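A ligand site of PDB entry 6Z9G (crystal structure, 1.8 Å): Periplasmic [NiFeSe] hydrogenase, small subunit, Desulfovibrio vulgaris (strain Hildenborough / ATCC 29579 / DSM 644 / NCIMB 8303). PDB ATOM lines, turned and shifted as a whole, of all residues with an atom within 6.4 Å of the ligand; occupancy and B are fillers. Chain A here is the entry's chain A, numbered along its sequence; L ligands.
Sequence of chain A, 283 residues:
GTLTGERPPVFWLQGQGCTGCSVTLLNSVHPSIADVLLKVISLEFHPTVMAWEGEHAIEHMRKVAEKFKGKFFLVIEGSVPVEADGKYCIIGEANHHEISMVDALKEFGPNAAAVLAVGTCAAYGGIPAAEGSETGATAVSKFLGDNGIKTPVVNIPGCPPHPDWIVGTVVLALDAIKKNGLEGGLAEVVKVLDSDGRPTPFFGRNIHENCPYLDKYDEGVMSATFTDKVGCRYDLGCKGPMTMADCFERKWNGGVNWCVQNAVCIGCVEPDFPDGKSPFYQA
The backbone NH (N) of Arg 233 sits close to a sulfur (S2) of the ligand, at 3.4 Å.
A ring nitrogen (ND1) of His 208 is bound to an iron atom (FE2) of the ligand.
N of Leu 214 lies close to S1 of the ligand (3.7 Å).
The side-chain sulfur (SG) of Cys 232 binds an iron atom (FE3) of the ligand (2.3 Å).
FE1 of the ligand is bound by SG of Cys 238 (2.3 Å).
An iron atom (FE4) of the ligand is bound by the side-chain sulfur of Cys 211 (2.3 Å).
The backbone carbonyl oxygen (O) of Tyr 213 lies close to a sulfur (S1) of the ligand, at 3.5 Å.
Tyr 217 touches the ligand (CB to S1, 3.7 Å).
Tyr 234 touches the ligand (CB to S4, 3.6 Å).
Gly 240 touches the ligand.
Pro 241 touches the ligand (CD to S4, 3.7 Å).
CG1 of Val 260 touches S2 of the ligand, 3.4 Å away.
Hydrophobic or aromatic side chains that line the ligand: His 208, Tyr 217, Tyr 234, Pro 241 and Val 260.
Of the 23 residues printed, 12 come within 4 Å of the ligand.
O of Gly 240 lies within hydrogen-bond range of N of His 208.
SG of Cys 232 lies close to N of Tyr 234, at 3.3 Å.
The side-chain sulfur of Cys 238 sits close to the backbone NH of Gly 240 (3.4 Å).
The side-chain sulfur (SG) of Cys 211 sits close to the backbone NH (N) of Tyr 213 (3.4 Å).
The backbone carbonyl oxygen of Gly 231 is in hydrogen-bond range of the guanidinium group of Arg 233, at 2.7 Å.
The side-chain sulfur (SG) of Cys 232 sits close to the side-chain sulfur (SD) of Met 222 (3.7 Å).
The backbone carbonyl oxygen of Arg 233 is in hydrogen-bond range of the backbone NH of Cys 238 (3.2 Å).
NE of Arg 233 sits at hydrogen-bond distance from O of Val 260 (2.8 Å).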
ATOM      1  N   ILE A 207     -21.785  -2.192   1.315  1.00  0.00           N
ATOM      2  CA  ILE A 207     -20.733  -3.000   1.946  1.00  0.00           C
ATOM      3  C   ILE A 207     -21.345  -4.024   2.893  1.00  0.00           C
ATOM      4  O   ILE A 207     -21.007  -5.221   2.849  1.00  0.00           O
ATOM      5  CB  ILE A 207     -19.703  -2.100   2.673  1.00  0.00           C
ATOM      6  CG1 ILE A 207     -18.823  -1.342   1.673  1.00  0.00           C
ATOM      7  CG2 ILE A 207     -18.825  -2.942   3.623  1.00  0.00           C
ATOM      8  CD1 ILE A 207     -17.802  -0.428   2.325  1.00  0.00           C
ATOM      9  N   HIS A 208     -22.255  -3.591   3.761  1.00  0.00           N
ATOM     10  CA  HIS A 208     -22.751  -4.474   4.813  1.00  0.00           C
ATOM     11  C   HIS A 208     -23.453  -5.682   4.214  1.00  0.00           C
ATOM     12  O   HIS A 208     -23.186  -6.819   4.593  1.00  0.00           O
ATOM     13  CB  HIS A 208     -23.683  -3.684   5.741  1.00  0.00           C
ATOM     14  CG  HIS A 208     -24.346  -4.532   6.785  1.00  0.00           C
ATOM     15  ND1 HIS A 208     -23.693  -4.976   7.913  1.00  0.00           N
ATOM     16  CD2 HIS A 208     -25.616  -5.006   6.874  1.00  0.00           C
ATOM     17  CE1 HIS A 208     -24.534  -5.692   8.648  1.00  0.00           C
ATOM     18  NE2 HIS A 208     -25.698  -5.720   8.038  1.00  0.00           N
ATOM     19  N   GLU A 209     -24.351  -5.437   3.256  1.00  0.00           N
ATOM     20  CA  GLU A 209     -25.082  -6.520   2.624  1.00  0.00           C
ATOM     21  C   GLU A 209     -24.144  -7.536   1.994  1.00  0.00           C
ATOM     22  O   GLU A 209     -24.580  -8.663   1.718  1.00  0.00           O
ATOM     23  CB  GLU A 209     -26.040  -5.949   1.578  1.00  0.00           C
ATOM     24  CG  GLU A 209     -27.176  -5.152   2.192  1.00  0.00           C
ATOM     25  CD  GLU A 209     -27.960  -4.359   1.168  1.00  0.00           C
ATOM     26  OE1 GLU A 209     -27.814  -4.623  -0.044  1.00  0.00           O
ATOM     27  OE2 GLU A 209     -28.732  -3.468   1.587  1.00  0.00           O
ATOM     28  N   CYS A 211     -20.896  -8.008   3.389  1.00  0.00           N
ATOM     29  CA  CYS A 211     -19.779  -8.126   4.293  1.00  0.00           C
ATOM     30  C   CYS A 211     -19.589  -9.579   4.727  1.00  0.00           C
ATOM     31  O   CYS A 211     -20.563 -10.255   5.049  1.00  0.00           O
ATOM     32  CB  CYS A 211     -19.976  -7.258   5.529  1.00  0.00           C
ATOM     33  SG  CYS A 211     -18.536  -7.324   6.615  1.00  0.00           S
ATOM     34  N   PRO A 212     -18.342 -10.065   4.787  1.00  0.00           N
ATOM     35  CA  PRO A 212     -18.110 -11.426   5.273  1.00  0.00           C
ATOM     36  C   PRO A 212     -18.388 -11.628   6.763  1.00  0.00           C
ATOM     37  O   PRO A 212     -18.398 -12.790   7.211  1.00  0.00           O
ATOM     38  CB  PRO A 212     -16.631 -11.674   4.950  1.00  0.00           C
ATOM     39  CG  PRO A 212     -16.022 -10.313   4.791  1.00  0.00           C
ATOM     40  CD  PRO A 212     -17.112  -9.422   4.265  1.00  0.00           C
ATOM     41  N   TYR A 213     -18.623 -10.569   7.530  1.00  0.00           N
ATOM     42  CA  TYR A 213     -19.009 -10.690   8.935  1.00  0.00           C
ATOM     43  C   TYR A 213     -20.508 -10.528   9.125  1.00  0.00           C
ATOM     44  O   TYR A 213     -20.982 -10.367  10.256  1.00  0.00           O
ATOM     45  CB  TYR A 213     -18.235  -9.688   9.804  1.00  0.00           C
ATOM     46  CG  TYR A 213     -16.752  -9.771   9.587  1.00  0.00           C
ATOM     47  CD1 TYR A 213     -16.039 -10.881  10.002  1.00  0.00           C
ATOM     48  CD2 TYR A 213     -16.054  -8.754   8.954  1.00  0.00           C
ATOM     49  CE1 TYR A 213     -14.691 -10.986   9.795  1.00  0.00           C
ATOM     50  CE2 TYR A 213     -14.697  -8.848   8.743  1.00  0.00           C
ATOM     51  CZ  TYR A 213     -14.017  -9.966   9.168  1.00  0.00           C
ATOM     52  OH  TYR A 213     -12.657 -10.074   8.973  1.00  0.00           O
ATOM     53  N   LEU A 214     -21.266 -10.616   8.028  1.00  0.00           N
ATOM     54  CA  LEU A 214     -22.710 -10.441   8.104  1.00  0.00           C
ATOM     55  C   LEU A 214     -23.361 -11.548   8.937  1.00  0.00           C
ATOM     56  O   LEU A 214     -24.377 -11.297   9.594  1.00  0.00           O
ATOM     57  CB  LEU A 214     -23.300 -10.421   6.696  1.00  0.00           C
ATOM     58  CG  LEU A 214     -24.788 -10.077   6.586  1.00  0.00           C
ATOM     59  CD1 LEU A 214     -25.027  -8.678   7.173  1.00  0.00           C
ATOM     60  CD2 LEU A 214     -25.262 -10.166   5.140  1.00  0.00           C
ATOM     61  N   ASP A 215     -22.795 -12.756   8.918  1.00  0.00           N
ATOM     62  CA  ASP A 215     -23.308 -13.839   9.755  1.00  0.00           C
ATOM     63  C   ASP A 215     -23.181 -13.482  11.242  1.00  0.00           C
ATOM     64  O   ASP A 215     -24.120 -13.666  12.013  1.00  0.00           O
ATOM     65  CB  ASP A 215     -22.559 -15.145   9.464  1.00  0.00           C
ATOM     66  CG  ASP A 215     -21.041 -15.006   9.602  1.00  0.00           C
ATOM     67  OD1 ASP A 215     -20.508 -13.891   9.461  1.00  0.00           O
ATOM     68  OD2 ASP A 215     -20.368 -16.022   9.867  1.00  0.00           O
ATOM     69  N   LYS A 216     -22.020 -12.969  11.635  1.00  0.00           N
ATOM     70  CA  LYS A 216     -21.823 -12.581  13.031  1.00  0.00           C
ATOM     71  C   LYS A 216     -22.759 -11.446  13.420  1.00  0.00           C
ATOM     72  O   LYS A 216     -23.310 -11.435  14.520  1.00  0.00           O
ATOM     73  CB  LYS A 216     -20.360 -12.192  13.274  1.00  0.00           C
ATOM     74  CG  LYS A 216     -19.353 -13.276  12.893  1.00  0.00           C
ATOM     75  CD  LYS A 216     -19.501 -14.492  13.797  1.00  0.00           C
ATOM     76  CE  LYS A 216     -18.535 -15.594  13.430  1.00  0.00           C
ATOM     77  NZ  LYS A 216     -18.763 -16.835  14.233  1.00  0.00           N
ATOM     78  N   TYR A 217     -22.928 -10.466  12.527  1.00  0.00           N
ATOM     79  CA  TYR A 217     -23.854  -9.367  12.780  1.00  0.00           C
ATOM     80  C   TYR A 217     -25.252  -9.877  13.088  1.00  0.00           C
ATOM     81  O   TYR A 217     -25.894  -9.414  14.045  1.00  0.00           O
ATOM     82  CB  TYR A 217     -23.899  -8.440  11.560  1.00  0.00           C
ATOM     83  CG  TYR A 217     -24.980  -7.383  11.638  1.00  0.00           C
ATOM     84  CD1 TYR A 217     -24.743  -6.152  12.242  1.00  0.00           C
ATOM     85  CD2 TYR A 217     -26.248  -7.622  11.121  1.00  0.00           C
ATOM     86  CE1 TYR A 217     -25.736  -5.175  12.298  1.00  0.00           C
ATOM     87  CE2 TYR A 217     -27.256  -6.662  11.177  1.00  0.00           C
ATOM     88  CZ  TYR A 217     -26.988  -5.440  11.774  1.00  0.00           C
ATOM     89  OH  TYR A 217     -27.980  -4.493  11.830  1.00  0.00           O
ATOM     90  N   MET A 222     -20.529  -9.477  18.398  1.00  0.00           N
ATOM     91  CA  MET A 222     -19.838  -8.213  18.164  1.00  0.00           C
ATOM     92  C   MET A 222     -18.443  -8.252  18.765  1.00  0.00           C
ATOM     93  O   MET A 222     -18.251  -8.774  19.864  1.00  0.00           O
ATOM     94  CB  MET A 222     -20.612  -7.049  18.781  1.00  0.00           C
ATOM     95  CG  MET A 222     -22.033  -6.896  18.290  1.00  0.00           C
ATOM     96  SD  MET A 222     -22.042  -6.403  16.554  1.00  0.00           S
ATOM     97  CE  MET A 222     -23.808  -6.231  16.267  1.00  0.00           C
ATOM     98  N   GLY A 231     -15.706 -11.200  15.624  1.00  0.00           N
ATOM     99  CA  GLY A 231     -17.027 -10.614  15.710  1.00  0.00           C
ATOM    100  C   GLY A 231     -17.273  -9.556  14.672  1.00  0.00           C
ATOM    101  O   GLY A 231     -16.370  -9.096  13.966  1.00  0.00           O
ATOM    102  N   CYS A 232     -18.540  -9.170  14.585  1.00  0.00           N
ATOM    103  CA  CYS A 232     -18.934  -8.042  13.750  1.00  0.00           C
ATOM    104  C   CYS A 232     -18.427  -6.741  14.358  1.00  0.00           C
ATOM    105  O   CYS A 232     -18.340  -6.591  15.586  1.00  0.00           O
ATOM    106  CB  CYS A 232     -20.444  -8.013  13.575  1.00  0.00           C
ATOM    107  SG  CYS A 232     -21.152  -6.487  12.947  1.00  0.00           S
ATOM    108  N   ARG A 233     -18.082  -5.791  13.495  1.00  0.00           N
ATOM    109  CA  ARG A 233     -17.492  -4.527  13.919  1.00  0.00           C
ATOM    110  C   ARG A 233     -18.524  -3.451  14.233  1.00  0.00           C
ATOM    111  O   ARG A 233     -18.149  -2.302  14.491  1.00  0.00           O
ATOM    112  CB  ARG A 233     -16.528  -4.020  12.845  1.00  0.00           C
ATOM    113  CG  ARG A 233     -15.191  -4.773  12.758  1.00  0.00           C
ATOM    114  CD  ARG A 233     -15.288  -6.223  12.267  1.00  0.00           C
ATOM    115  NE  ARG A 233     -14.003  -6.649  11.733  1.00  0.00           N
ATOM    116  CZ  ARG A 233     -13.535  -7.899  11.748  1.00  0.00           C
ATOM    117  NH1 ARG A 233     -14.235  -8.866  12.312  1.00  0.00           N
ATOM    118  NH2 ARG A 233     -12.341  -8.155  11.217  1.00  0.00           N
ATOM    119  N   TYR A 234     -19.808  -3.796  14.263  1.00  0.00           N
ATOM    120  CA  TYR A 234     -20.850  -2.772  14.360  1.00  0.00           C
ATOM    121  C   TYR A 234     -20.742  -1.951  15.638  1.00  0.00           C
ATOM    122  O   TYR A 234     -20.881  -0.727  15.603  1.00  0.00           O
ATOM    123  CB  TYR A 234     -22.238  -3.414  14.253  1.00  0.00           C
ATOM    124  CG  TYR A 234     -23.327  -2.368  14.358  1.00  0.00           C
ATOM    125  CD1 TYR A 234     -23.692  -1.617  13.264  1.00  0.00           C
ATOM    126  CD2 TYR A 234     -23.978  -2.129  15.563  1.00  0.00           C
ATOM    127  CE1 TYR A 234     -24.675  -0.660  13.337  1.00  0.00           C
ATOM    128  CE2 TYR A 234     -24.973  -1.173  15.655  1.00  0.00           C
ATOM    129  CZ  TYR A 234     -25.317  -0.440  14.537  1.00  0.00           C
ATOM    130  OH  TYR A 234     -26.302   0.512  14.619  1.00  0.00           O
ATOM    131  N   ASP A 235     -20.546  -2.612  16.779  1.00  0.00           N
ATOM    132  CA  ASP A 235     -20.490  -1.864  18.034  1.00  0.00           C
ATOM    133  C   ASP A 235     -19.239  -0.995  18.122  1.00  0.00           C
ATOM    134  O   ASP A 235     -19.256   0.033  18.825  1.00  0.00           O
ATOM    135  CB  ASP A 235     -20.563  -2.820  19.230  1.00  0.00           C
ATOM    136  CG  ASP A 235     -21.990  -3.270  19.534  1.00  0.00           C
ATOM    137  OD1 ASP A 235     -22.937  -2.645  19.010  1.00  0.00           O
ATOM    138  OD2 ASP A 235     -22.171  -4.246  20.285  1.00  0.00           O
ATOM    139  N   CYS A 238     -18.715   0.537  13.023  1.00  0.00           N
ATOM    140  CA  CYS A 238     -18.712   0.267  11.588  1.00  0.00           C
ATOM    141  C   CYS A 238     -19.923   0.889  10.910  1.00  0.00           C
ATOM    142  O   CYS A 238     -21.062   0.662  11.325  1.00  0.00           O
ATOM    143  CB  CYS A 238     -18.681  -1.241  11.322  1.00  0.00           C
ATOM    144  SG  CYS A 238     -18.569  -1.656   9.539  1.00  0.00           S
ATOM    145  N   LYS A 239     -19.687   1.681   9.869  1.00  0.00           N
ATOM    146  CA  LYS A 239     -20.737   2.303   9.090  1.00  0.00           C
ATOM    147  C   LYS A 239     -21.009   1.568   7.792  1.00  0.00           C
ATOM    148  O   LYS A 239     -21.675   2.112   6.907  1.00  0.00           O
ATOM    149  CB  LYS A 239     -20.397   3.764   8.786  1.00  0.00           C
ATOM    150  CG  LYS A 239     -20.135   4.620  10.010  1.00  0.00           C
ATOM    151  CD  LYS A 239     -21.242   4.492  11.029  1.00  0.00           C
ATOM    152  CE  LYS A 239     -21.035   5.460  12.185  1.00  0.00           C
ATOM    153  NZ  LYS A 239     -19.805   5.148  12.936  1.00  0.00           N
ATOM    154  N   GLY A 240     -20.495   0.341   7.649  1.00  0.00           N
ATOM    155  CA  GLY A 240     -20.790  -0.500   6.512  1.00  0.00           C
ATOM    156  C   GLY A 240     -22.269  -0.523   6.154  1.00  0.00           C
ATOM    157  O   GLY A 240     -22.634  -0.433   4.986  1.00  0.00           O
ATOM    158  N   PRO A 241     -23.145  -0.671   7.161  1.00  0.00           N
ATOM    159  CA  PRO A 241     -24.584  -0.698   6.846  1.00  0.00           C
ATOM    160  C   PRO A 241     -25.091   0.535   6.092  1.00  0.00           C
ATOM    161  O   PRO A 241     -26.138   0.433   5.438  1.00  0.00           O
ATOM    162  CB  PRO A 241     -25.240  -0.826   8.239  1.00  0.00           C
ATOM    163  CG  PRO A 241     -24.247  -1.640   9.020  1.00  0.00           C
ATOM    164  CD  PRO A 241     -22.878  -1.132   8.534  1.00  0.00           C
ATOM    165  N   TRP A 258      -8.559  -4.328   4.013  1.00  0.00           N
ATOM    166  CA  TRP A 258      -9.576  -3.309   3.844  1.00  0.00           C
ATOM    167  C   TRP A 258     -10.080  -2.898   5.223  1.00  0.00           C
ATOM    168  O   TRP A 258      -9.768  -3.533   6.239  1.00  0.00           O
ATOM    169  CB  TRP A 258     -10.698  -3.783   2.905  1.00  0.00           C
ATOM    170  CG  TRP A 258     -11.578  -4.851   3.432  1.00  0.00           C
ATOM    171  CD1 TRP A 258     -11.211  -6.120   3.826  1.00  0.00           C
ATOM    172  CD2 TRP A 258     -12.993  -4.760   3.614  1.00  0.00           C
ATOM    173  NE1 TRP A 258     -12.325  -6.801   4.253  1.00  0.00           N
ATOM    174  CE2 TRP A 258     -13.425  -5.994   4.126  1.00  0.00           C
ATOM    175  CE3 TRP A 258     -13.932  -3.754   3.405  1.00  0.00           C
ATOM    176  CZ2 TRP A 258     -14.763  -6.244   4.418  1.00  0.00           C
ATOM    177  CZ3 TRP A 258     -15.257  -4.004   3.701  1.00  0.00           C
ATOM    178  CH2 TRP A 258     -15.663  -5.237   4.199  1.00  0.00           C
ATOM    179  N   VAL A 260     -12.809  -2.781   7.086  1.00  0.00           N
ATOM    180  CA  VAL A 260     -13.601  -3.554   8.036  1.00  0.00           C
ATOM    181  C   VAL A 260     -12.782  -4.681   8.642  1.00  0.00           C
ATOM    182  O   VAL A 260     -12.902  -4.977   9.843  1.00  0.00           O
ATOM    183  CB  VAL A 260     -14.886  -4.076   7.357  1.00  0.00           C
ATOM    184  CG1 VAL A 260     -15.695  -4.964   8.319  1.00  0.00           C
ATOM    185  CG2 VAL A 260     -15.738  -2.906   6.861  1.00  0.00           C
ATOM    186  N   CYS A 265     -15.238   0.493   8.935  1.00  0.00           N
ATOM    187  CA  CYS A 265     -15.577   1.385   7.843  1.00  0.00           C
ATOM    188  C   CYS A 265     -16.097   2.700   8.416  1.00  0.00           C
ATOM    189  O   CYS A 265     -16.878   2.718   9.365  1.00  0.00           O
ATOM    190  CB  CYS A 265     -16.623   0.718   6.931  1.00  0.00           C
ATOM    191  SG  CYS A 265     -17.273   1.765   5.582  1.00  0.00           S
HETATM  192 FE1  LIG L   1     -19.761  -3.664   9.557  1.00  0.00          FE
HETATM  193 FE2  LIG L   1     -21.968  -4.827   8.688  1.00  0.00          FE
HETATM  194 FE3  LIG L   1     -20.684  -5.899  10.801  1.00  0.00          FE
HETATM  195 FE4  LIG L   1     -19.652  -6.089   8.214  1.00  0.00          FE
HETATM  196  S1  LIG L   1     -21.565  -7.091   9.031  1.00  0.00           S
HETATM  197  S2  LIG L   1     -18.513  -5.509  10.140  1.00  0.00           S
HETATM  198  S3  LIG L   1     -20.276  -4.082   7.348  1.00  0.00           S
HETATM  199  S4  LIG L   1     -21.713  -3.865  10.756  1.00  0.00           S
